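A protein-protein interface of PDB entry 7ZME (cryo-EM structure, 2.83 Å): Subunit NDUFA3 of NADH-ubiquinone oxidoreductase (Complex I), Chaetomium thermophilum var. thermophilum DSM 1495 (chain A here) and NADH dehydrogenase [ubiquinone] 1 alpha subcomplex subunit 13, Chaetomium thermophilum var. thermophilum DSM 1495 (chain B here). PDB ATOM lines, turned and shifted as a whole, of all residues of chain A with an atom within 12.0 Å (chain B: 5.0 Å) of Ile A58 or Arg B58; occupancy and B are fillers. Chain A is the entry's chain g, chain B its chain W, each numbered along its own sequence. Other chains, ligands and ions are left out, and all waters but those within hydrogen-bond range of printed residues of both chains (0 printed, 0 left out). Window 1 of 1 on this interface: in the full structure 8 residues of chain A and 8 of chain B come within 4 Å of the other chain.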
ATOM      1  N   ARG A  47      -4.667   7.281  -9.342  1.00  0.00           N
ATOM      2  CA  ARG A  47      -4.988   7.140  -7.900  1.00  0.00           C
ATOM      3  C   ARG A  47      -4.573   8.417  -7.178  1.00  0.00           C
ATOM      4  O   ARG A  47      -5.294   8.856  -6.294  1.00  0.00           O
ATOM      5  CB  ARG A  47      -4.341   5.883  -7.315  1.00  0.00           C
ATOM      6  CG  ARG A  47      -5.274   4.688  -7.222  1.00  0.00           C
ATOM      7  CD  ARG A  47      -4.761   3.582  -6.324  1.00  0.00           C
ATOM      8  NE  ARG A  47      -4.477   3.978  -4.952  1.00  0.00           N
ATOM      9  CZ  ARG A  47      -3.264   4.102  -4.427  1.00  0.00           C
ATOM     10  NH1 ARG A  47      -3.123   4.474  -3.168  1.00  0.00           N
ATOM     11  NH2 ARG A  47      -2.194   3.851  -5.159  1.00  0.00           N
ATOM     12  N   ASP A  52      -6.282   9.558  -3.895  1.00  0.00           N
ATOM     13  CA  ASP A  52      -5.979   8.319  -3.125  1.00  0.00           C
ATOM     14  C   ASP A  52      -4.517   8.400  -2.710  1.00  0.00           C
ATOM     15  O   ASP A  52      -3.665   8.598  -3.586  1.00  0.00           O
ATOM     16  CB  ASP A  52      -6.252   7.042  -3.918  1.00  0.00           C
ATOM     17  CG  ASP A  52      -6.599   5.851  -3.053  1.00  0.00           C
ATOM     18  OD1 ASP A  52      -6.352   5.920  -1.836  1.00  0.00           O
ATOM     19  OD2 ASP A  52      -7.125   4.875  -3.604  1.00  0.00           O
ATOM     20  N   VAL A  53      -4.257   8.326  -1.409  1.00  0.00           N
ATOM     21  CA  VAL A  53      -2.867   8.487  -0.917  1.00  0.00           C
ATOM     22  C   VAL A  53      -2.356   7.129  -0.456  1.00  0.00           C
ATOM     23  O   VAL A  53      -3.050   6.487   0.343  1.00  0.00           O
ATOM     24  CB  VAL A  53      -2.808   9.529   0.215  1.00  0.00           C
ATOM     25  CG1 VAL A  53      -1.412   9.658   0.803  1.00  0.00           C
ATOM     26  CG2 VAL A  53      -3.311  10.889  -0.241  1.00  0.00           C
ATOM     27  N   ASP A  54      -1.182   6.719  -0.928  1.00  0.00           N
ATOM     28  CA  ASP A  54      -0.562   5.473  -0.419  1.00  0.00           C
ATOM     29  C   ASP A  54      -0.345   5.725   1.072  1.00  0.00           C
ATOM     30  O   ASP A  54       0.101   6.830   1.419  1.00  0.00           O
ATOM     31  CB  ASP A  54       0.743   5.228  -1.178  1.00  0.00           C
ATOM     32  CG  ASP A  54       1.552   3.995  -0.807  1.00  0.00           C
ATOM     33  OD1 ASP A  54       1.487   3.563   0.353  1.00  0.00           O
ATOM     34  OD2 ASP A  54       2.261   3.480  -1.694  1.00  0.00           O
ATOM     35  N   ALA A  55      -0.653   4.741   1.917  1.00  0.00           N
ATOM     36  CA  ALA A  55      -0.536   4.942   3.374  1.00  0.00           C
ATOM     37  C   ALA A  55       0.929   4.923   3.784  1.00  0.00           C
ATOM     38  O   ALA A  55       1.765   4.479   2.980  1.00  0.00           O
ATOM     39  CB  ALA A  55      -1.322   3.887   4.100  1.00  0.00           C
ATOM     40  N   ALA A  56       1.225   5.414   4.983  1.00  0.00           N
ATOM     41  CA  ALA A  56       2.599   5.346   5.523  1.00  0.00           C
ATOM     42  C   ALA A  56       2.887   3.914   5.975  1.00  0.00           C
ATOM     43  O   ALA A  56       1.959   3.248   6.447  1.00  0.00           O
ATOM     44  CB  ALA A  56       2.708   6.298   6.672  1.00  0.00           C
ATOM     45  N   PRO A  57       4.123   3.400   5.837  1.00  0.00           N
ATOM     46  CA  PRO A  57       4.446   2.071   6.342  1.00  0.00           C
ATOM     47  C   PRO A  57       4.197   1.867   7.851  1.00  0.00           C
ATOM     48  O   PRO A  57       4.508   2.753   8.615  1.00  0.00           O
ATOM     49  CB  PRO A  57       5.931   1.927   5.988  1.00  0.00           C
ATOM     50  CG  PRO A  57       6.423   3.342   5.809  1.00  0.00           C
ATOM     51  CD  PRO A  57       5.250   4.062   5.186  1.00  0.00           C
ATOM     52  N   ILE A  58       3.668   0.701   8.242  1.00  0.00           N
ATOM     53  CA  ILE A  58       3.470   0.389   9.689  1.00  0.00           C
ATOM     54  C   ILE A  58       4.836   0.125  10.349  1.00  0.00           C
ATOM     55  O   ILE A  58       5.705  -0.424   9.658  1.00  0.00           O
ATOM     56  CB  ILE A  58       2.473  -0.766   9.918  1.00  0.00           C
ATOM     57  CG1 ILE A  58       3.062  -2.133   9.558  1.00  0.00           C
ATOM     58  CG2 ILE A  58       1.163  -0.501   9.195  1.00  0.00           C
ATOM     59  CD1 ILE A  58       2.389  -3.283  10.255  1.00  0.00           C
ATOM     60  N   PRO A  59       5.113   0.516  11.620  1.00  0.00           N
ATOM     61  CA  PRO A  59       6.452   0.312  12.187  1.00  0.00           C
ATOM     62  C   PRO A  59       6.715  -1.158  12.477  1.00  0.00           C
ATOM     63  O   PRO A  59       5.942  -1.818  13.173  1.00  0.00           O
ATOM     64  CB  PRO A  59       6.423   1.147  13.472  1.00  0.00           C
ATOM     65  CG  PRO A  59       4.990   1.269  13.815  1.00  0.00           C
ATOM     66  CD  PRO A  59       4.234   1.269  12.528  1.00  0.00           C
ATOM     67  N   LEU A  60       7.848  -1.661  12.006  1.00  0.00           N
ATOM     68  CA  LEU A  60       8.225  -3.083  12.223  1.00  0.00           C
ATOM     69  C   LEU A  60       9.512  -3.118  13.047  1.00  0.00           C
ATOM     70  O   LEU A  60      10.141  -4.169  13.081  1.00  0.00           O
ATOM     71  CB  LEU A  60       8.355  -3.779  10.866  1.00  0.00           C
ATOM     72  CG  LEU A  60       7.105  -3.746   9.990  1.00  0.00           C
ATOM     73  CD1 LEU A  60       7.370  -4.391   8.644  1.00  0.00           C
ATOM     74  CD2 LEU A  60       5.955  -4.437  10.690  1.00  0.00           C
ATOM     75  N   THR A  61       9.836  -2.025  13.737  1.00  0.00           N
ATOM     76  CA  THR A  61      10.982  -1.917  14.679  1.00  0.00           C
ATOM     77  C   THR A  61      10.620  -0.729  15.572  1.00  0.00           C
ATOM     78  O   THR A  61       9.766   0.053  15.152  1.00  0.00           O
ATOM     79  CB  THR A  61      12.340  -1.706  13.985  1.00  0.00           C
ATOM     80  OG1 THR A  61      13.384  -1.857  14.944  1.00  0.00           O
ATOM     81  CG2 THR A  61      12.475  -0.365  13.300  1.00  0.00           C
ATOM     82  N   TYR A  62      11.121  -0.687  16.805  1.00  0.00           N
ATOM     83  CA  TYR A  62      10.843   0.468  17.689  1.00  0.00           C
ATOM     84  C   TYR A  62      11.289   1.742  16.978  1.00  0.00           C
ATOM     85  O   TYR A  62      12.436   1.822  16.518  1.00  0.00           O
ATOM     86  CB  TYR A  62      11.551   0.326  19.037  1.00  0.00           C
ATOM     87  CG  TYR A  62      11.099   1.311  20.084  1.00  0.00           C
ATOM     88  CD1 TYR A  62      11.610   2.597  20.132  1.00  0.00           C
ATOM     89  CD2 TYR A  62      10.149   0.957  21.026  1.00  0.00           C
ATOM     90  CE1 TYR A  62      11.184   3.510  21.080  1.00  0.00           C
ATOM     91  CE2 TYR A  62       9.720   1.854  21.986  1.00  0.00           C
ATOM     92  CZ  TYR A  62      10.239   3.135  22.015  1.00  0.00           C
ATOM     93  OH  TYR A  62       9.819   4.017  22.963  1.00  0.00           O
ATOM     94  N   PRO A  63      10.418   2.766  16.897  1.00  0.00           N
ATOM     95  CA  PRO A  63      10.748   4.000  16.199  1.00  0.00           C
ATOM     96  C   PRO A  63      11.654   4.848  17.095  1.00  0.00           C
ATOM     97  O   PRO A  63      11.139   5.540  17.939  1.00  0.00           O
ATOM     98  CB  PRO A  63       9.381   4.666  16.006  1.00  0.00           C
ATOM     99  CG  PRO A  63       8.368   3.608  16.378  1.00  0.00           C
ATOM    100  CD  PRO A  63       9.061   2.774  17.428  1.00  0.00           C
ATOM    101  N   ILE A  64      12.968   4.767  16.890  1.00  0.00           N
ATOM    102  CA  ILE A  64      13.910   5.481  17.792  1.00  0.00           C
ATOM    103  C   ILE A  64      13.916   6.955  17.389  1.00  0.00           C
ATOM    104  O   ILE A  64      14.249   7.219  16.224  1.00  0.00           O
ATOM    105  CB  ILE A  64      15.317   4.856  17.790  1.00  0.00           C
ATOM    106  CG1 ILE A  64      15.290   3.368  18.147  1.00  0.00           C
ATOM    107  CG2 ILE A  64      16.241   5.633  18.715  1.00  0.00           C
ATOM    108  CD1 ILE A  64      15.299   3.097  19.628  1.00  0.00           C
ATOM    109  N   ASN B  54      -4.427  -3.277   7.233  1.00  0.00           N
ATOM    110  CA  ASN B  54      -3.096  -2.634   7.329  1.00  0.00           C
ATOM    111  C   ASN B  54      -3.178  -1.562   8.409  1.00  0.00           C
ATOM    112  O   ASN B  54      -2.155  -1.327   9.064  1.00  0.00           O
ATOM    113  CB  ASN B  54      -2.575  -2.171   5.964  1.00  0.00           C
ATOM    114  CG  ASN B  54      -2.208  -3.317   5.046  1.00  0.00           C
ATOM    115  OD1 ASN B  54      -2.294  -4.481   5.429  1.00  0.00           O
ATOM    116  ND2 ASN B  54      -1.797  -3.000   3.832  1.00  0.00           N
ATOM    117  N   GLU B  55      -4.344  -0.933   8.571  1.00  0.00           N
ATOM    118  CA  GLU B  55      -4.561   0.052   9.662  1.00  0.00           C
ATOM    119  C   GLU B  55      -4.678  -0.641  11.025  1.00  0.00           C
ATOM    120  O   GLU B  55      -4.150  -0.092  12.000  1.00  0.00           O
ATOM    121  CB  GLU B  55      -5.719   0.970   9.287  1.00  0.00           C
ATOM    122  CG  GLU B  55      -5.376   1.890   8.136  1.00  0.00           C
ATOM    123  CD  GLU B  55      -3.988   2.495   8.252  1.00  0.00           C
ATOM    124  OE1 GLU B  55      -3.188   2.329   7.310  1.00  0.00           O
ATOM    125  OE2 GLU B  55      -3.713   3.140   9.281  1.00  0.00           O
ATOM    126  N   LEU B  56      -5.354  -1.784  11.100  1.00  0.00           N
ATOM    127  CA  LEU B  56      -5.452  -2.578  12.352  1.00  0.00           C
ATOM    128  C   LEU B  56      -4.051  -3.037  12.745  1.00  0.00           C
ATOM    129  O   LEU B  56      -3.780  -3.111  13.952  1.00  0.00           O
ATOM    130  CB  LEU B  56      -6.348  -3.789  12.081  1.00  0.00           C
ATOM    131  CG  LEU B  56      -7.841  -3.510  11.940  1.00  0.00           C
ATOM    132  CD1 LEU B  56      -8.594  -4.802  11.684  1.00  0.00           C
ATOM    133  CD2 LEU B  56      -8.375  -2.826  13.182  1.00  0.00           C
ATOM    134  N   ALA B  57      -3.226  -3.383  11.757  1.00  0.00           N
ATOM    135  CA  ALA B  57      -1.825  -3.792  12.002  1.00  0.00           C
ATOM    136  C   ALA B  57      -1.031  -2.633  12.606  1.00  0.00           C
ATOM    137  O   ALA B  57      -0.179  -2.901  13.459  1.00  0.00           O
ATOM    138  CB  ALA B  57      -1.218  -4.295  10.724  1.00  0.00           C
ATOM    139  N   ARG B  58      -1.290  -1.400  12.164  1.00  0.00           N
ATOM    140  CA  ARG B  58      -0.604  -0.200  12.714  1.00  0.00           C
ATOM    141  C   ARG B  58      -0.957  -0.024  14.190  1.00  0.00           C
ATOM    142  O   ARG B  58      -0.060   0.315  14.967  1.00  0.00           O
ATOM    143  CB  ARG B  58      -1.005   1.036  11.909  1.00  0.00           C
ATOM    144  CG  ARG B  58      -0.275   2.309  12.308  1.00  0.00           C
ATOM    145  CD  ARG B  58      -0.845   3.535  11.623  1.00  0.00           C
ATOM    146  NE  ARG B  58      -1.074   3.308  10.206  1.00  0.00           N
ATOM    147  CZ  ARG B  58      -0.167   3.474   9.253  1.00  0.00           C
ATOM    148  NH1 ARG B  58      -0.489   3.236   7.995  1.00  0.00           N
ATOM    149  NH2 ARG B  58       1.054   3.876   9.555  1.00  0.00           N
ATOM    150  N   GLU B  59      -2.209  -0.281  14.565  1.00  0.00           N
ATOM    151  CA  GLU B  59      -2.673  -0.116  15.964  1.00  0.00           C
ATOM    152  C   GLU B  59      -2.034  -1.186  16.848  1.00  0.00           C
ATOM    153  O   GLU B  59      -1.601  -0.837  17.953  1.00  0.00           O
ATOM    154  CB  GLU B  59      -4.196  -0.066  15.973  1.00  0.00           C
ATOM    155  CG  GLU B  59      -4.816   0.031  17.350  1.00  0.00           C
ATOM    156  CD  GLU B  59      -6.322  -0.127  17.301  1.00  0.00           C
ATOM    157  OE1 GLU B  59      -6.847  -0.335  16.198  1.00  0.00           O
ATOM    158  OE2 GLU B  59      -6.963  -0.058  18.359  1.00  0.00           O
ATOM    159  N   LYS B  60      -1.971  -2.431  16.370  1.00  0.00           N
ATOM    160  CA  LYS B  60      -1.355  -3.559  17.129  1.00  0.00           C
ATOM    161  C   LYS B  60       0.129  -3.284  17.356  1.00  0.00           C
ATOM    162  O   LYS B  60       0.644  -3.709  18.390  1.00  0.00           O
ATOM    163  CB  LYS B  60      -1.504  -4.870  16.357  1.00  0.00           C
ATOM    164  CG  LYS B  60      -1.010  -6.112  17.082  1.00  0.00           C
ATOM    165  CD  LYS B  60      -1.296  -7.389  16.339  1.00  0.00           C
ATOM    166  CE  LYS B  60      -1.019  -8.616  17.176  1.00  0.00           C
ATOM    167  NZ  LYS B  60      -1.597  -9.831  16.560  1.00  0.00           N
ATOM    168  N   MET B  61       0.777  -2.576  16.432  1.00  0.00           N
ATOM    169  CA  MET B  61       2.237  -2.365  16.534  1.00  0.00           C
ATOM    170  C   MET B  61       2.530  -1.191  17.467  1.00  0.00           C
ATOM    171  O   MET B  61       3.477  -1.321  18.238  1.00  0.00           O
ATOM    172  CB  MET B  61       2.871  -2.136  15.159  1.00  0.00           C
ATOM    173  CG  MET B  61       2.927  -3.377  14.283  1.00  0.00           C
ATOM    174  SD  MET B  61       3.921  -4.736  14.954  1.00  0.00           S
ATOM    175  CE  MET B  61       2.647  -5.838  15.564  1.00  0.00           C
ATOM    176  N   TRP B  62       1.727  -0.123  17.434  1.00  0.00           N
ATOM    177  CA  TRP B  62       1.926   1.017  18.367  1.00  0.00           C
ATOM    178  C   TRP B  62       1.607   0.601  19.802  1.00  0.00           C
ATOM    179  O   TRP B  62       2.301   1.069  20.698  1.00  0.00           O
ATOM    180  CB  TRP B  62       1.209   2.282  17.888  1.00  0.00           C
ATOM    181  CG  TRP B  62       2.003   3.018  16.856  1.00  0.00           C
ATOM    182  CD1 TRP B  62       1.794   3.041  15.509  1.00  0.00           C
ATOM    183  CD2 TRP B  62       3.178   3.809  17.093  1.00  0.00           C
ATOM    184  NE1 TRP B  62       2.744   3.809  14.895  1.00  0.00           N
ATOM    185  CE2 TRP B  62       3.611   4.288  15.840  1.00  0.00           C
ATOM    186  CE3 TRP B  62       3.896   4.166  18.240  1.00  0.00           C
ATOM    187  CZ2 TRP B  62       4.729   5.107  15.706  1.00  0.00           C
ATOM    188  CZ3 TRP B  62       5.000   4.976  18.104  1.00  0.00           C
ATOM    189  CH2 TRP B  62       5.406   5.441  16.855  1.00  0.00           C
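The backbone carbonyl oxygen (O) of Ala A56 is in hydrogen-bond range of the guanidinium group (NH1) of Arg B58.
The side-chain carboxylate of Glu B55 lies within salt-bridge range of the guanidinium group of Arg B58 (2.8 Å).
Among the printed residues, pairs that only touch across the chains: Ile A58 with Asn B54 (3.4 Å), Pro A63 with Trp B62 (3.5 Å), Pro A59 with Trp B62 (3.6 Å), Pro A59 with Met B61 (3.6 Å), Pro A57 with Arg B58 (3.8 Å), Ile A58 with Ala B57 (3.8 Å) and Ile A58 with Arg B58 (3.8 Å).
Printed residues of chain B within 4 Å of Ile A58: Asn B54 (3.4 Å), Ala B57 (3.8 Å) and Arg B58 (3.8 Å). Arg B58 touches just these residues of chain A: Ala A56, Pro A57 and Ile A58. Of chain A, only Ile A58 comes within 4 Å of Asn B54. No residue of chain A comes within 4 Å of Glu B55. Ala B57 touches one residue of chain A. Of chain A, only Pro A59 comes within 4 Å of Met B61. Of the printed residues of chain B, Pro A59 touches Met B61 and Trp B62. Of the printed residues of chain B, Pro A57 touches Arg B58. Of the printed residues of chain B, Pro A63 touches Trp B62. Of the printed residues of chain B, Ala A56 touches Arg B58 (2.9 Å).
Printed residues of chain B that touch a printed residue of chain A: Asn B54, Ala B57, Arg B58, Met B61 and Trp B62. Hydrophobic or aromatic side chains of chain B within 4 Å of the printed part of chain A: Ala B57, Met B61 and Trp B62. Hydrophobic or aromatic side chains of chain A that line the printed part of chain B: Ile A58, Pro A59 and Pro A63. Among the printed residues, no Asp or Glu carboxylate lies within 4 Å of a Lys or Arg side-chain nitrogen of the other chain.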
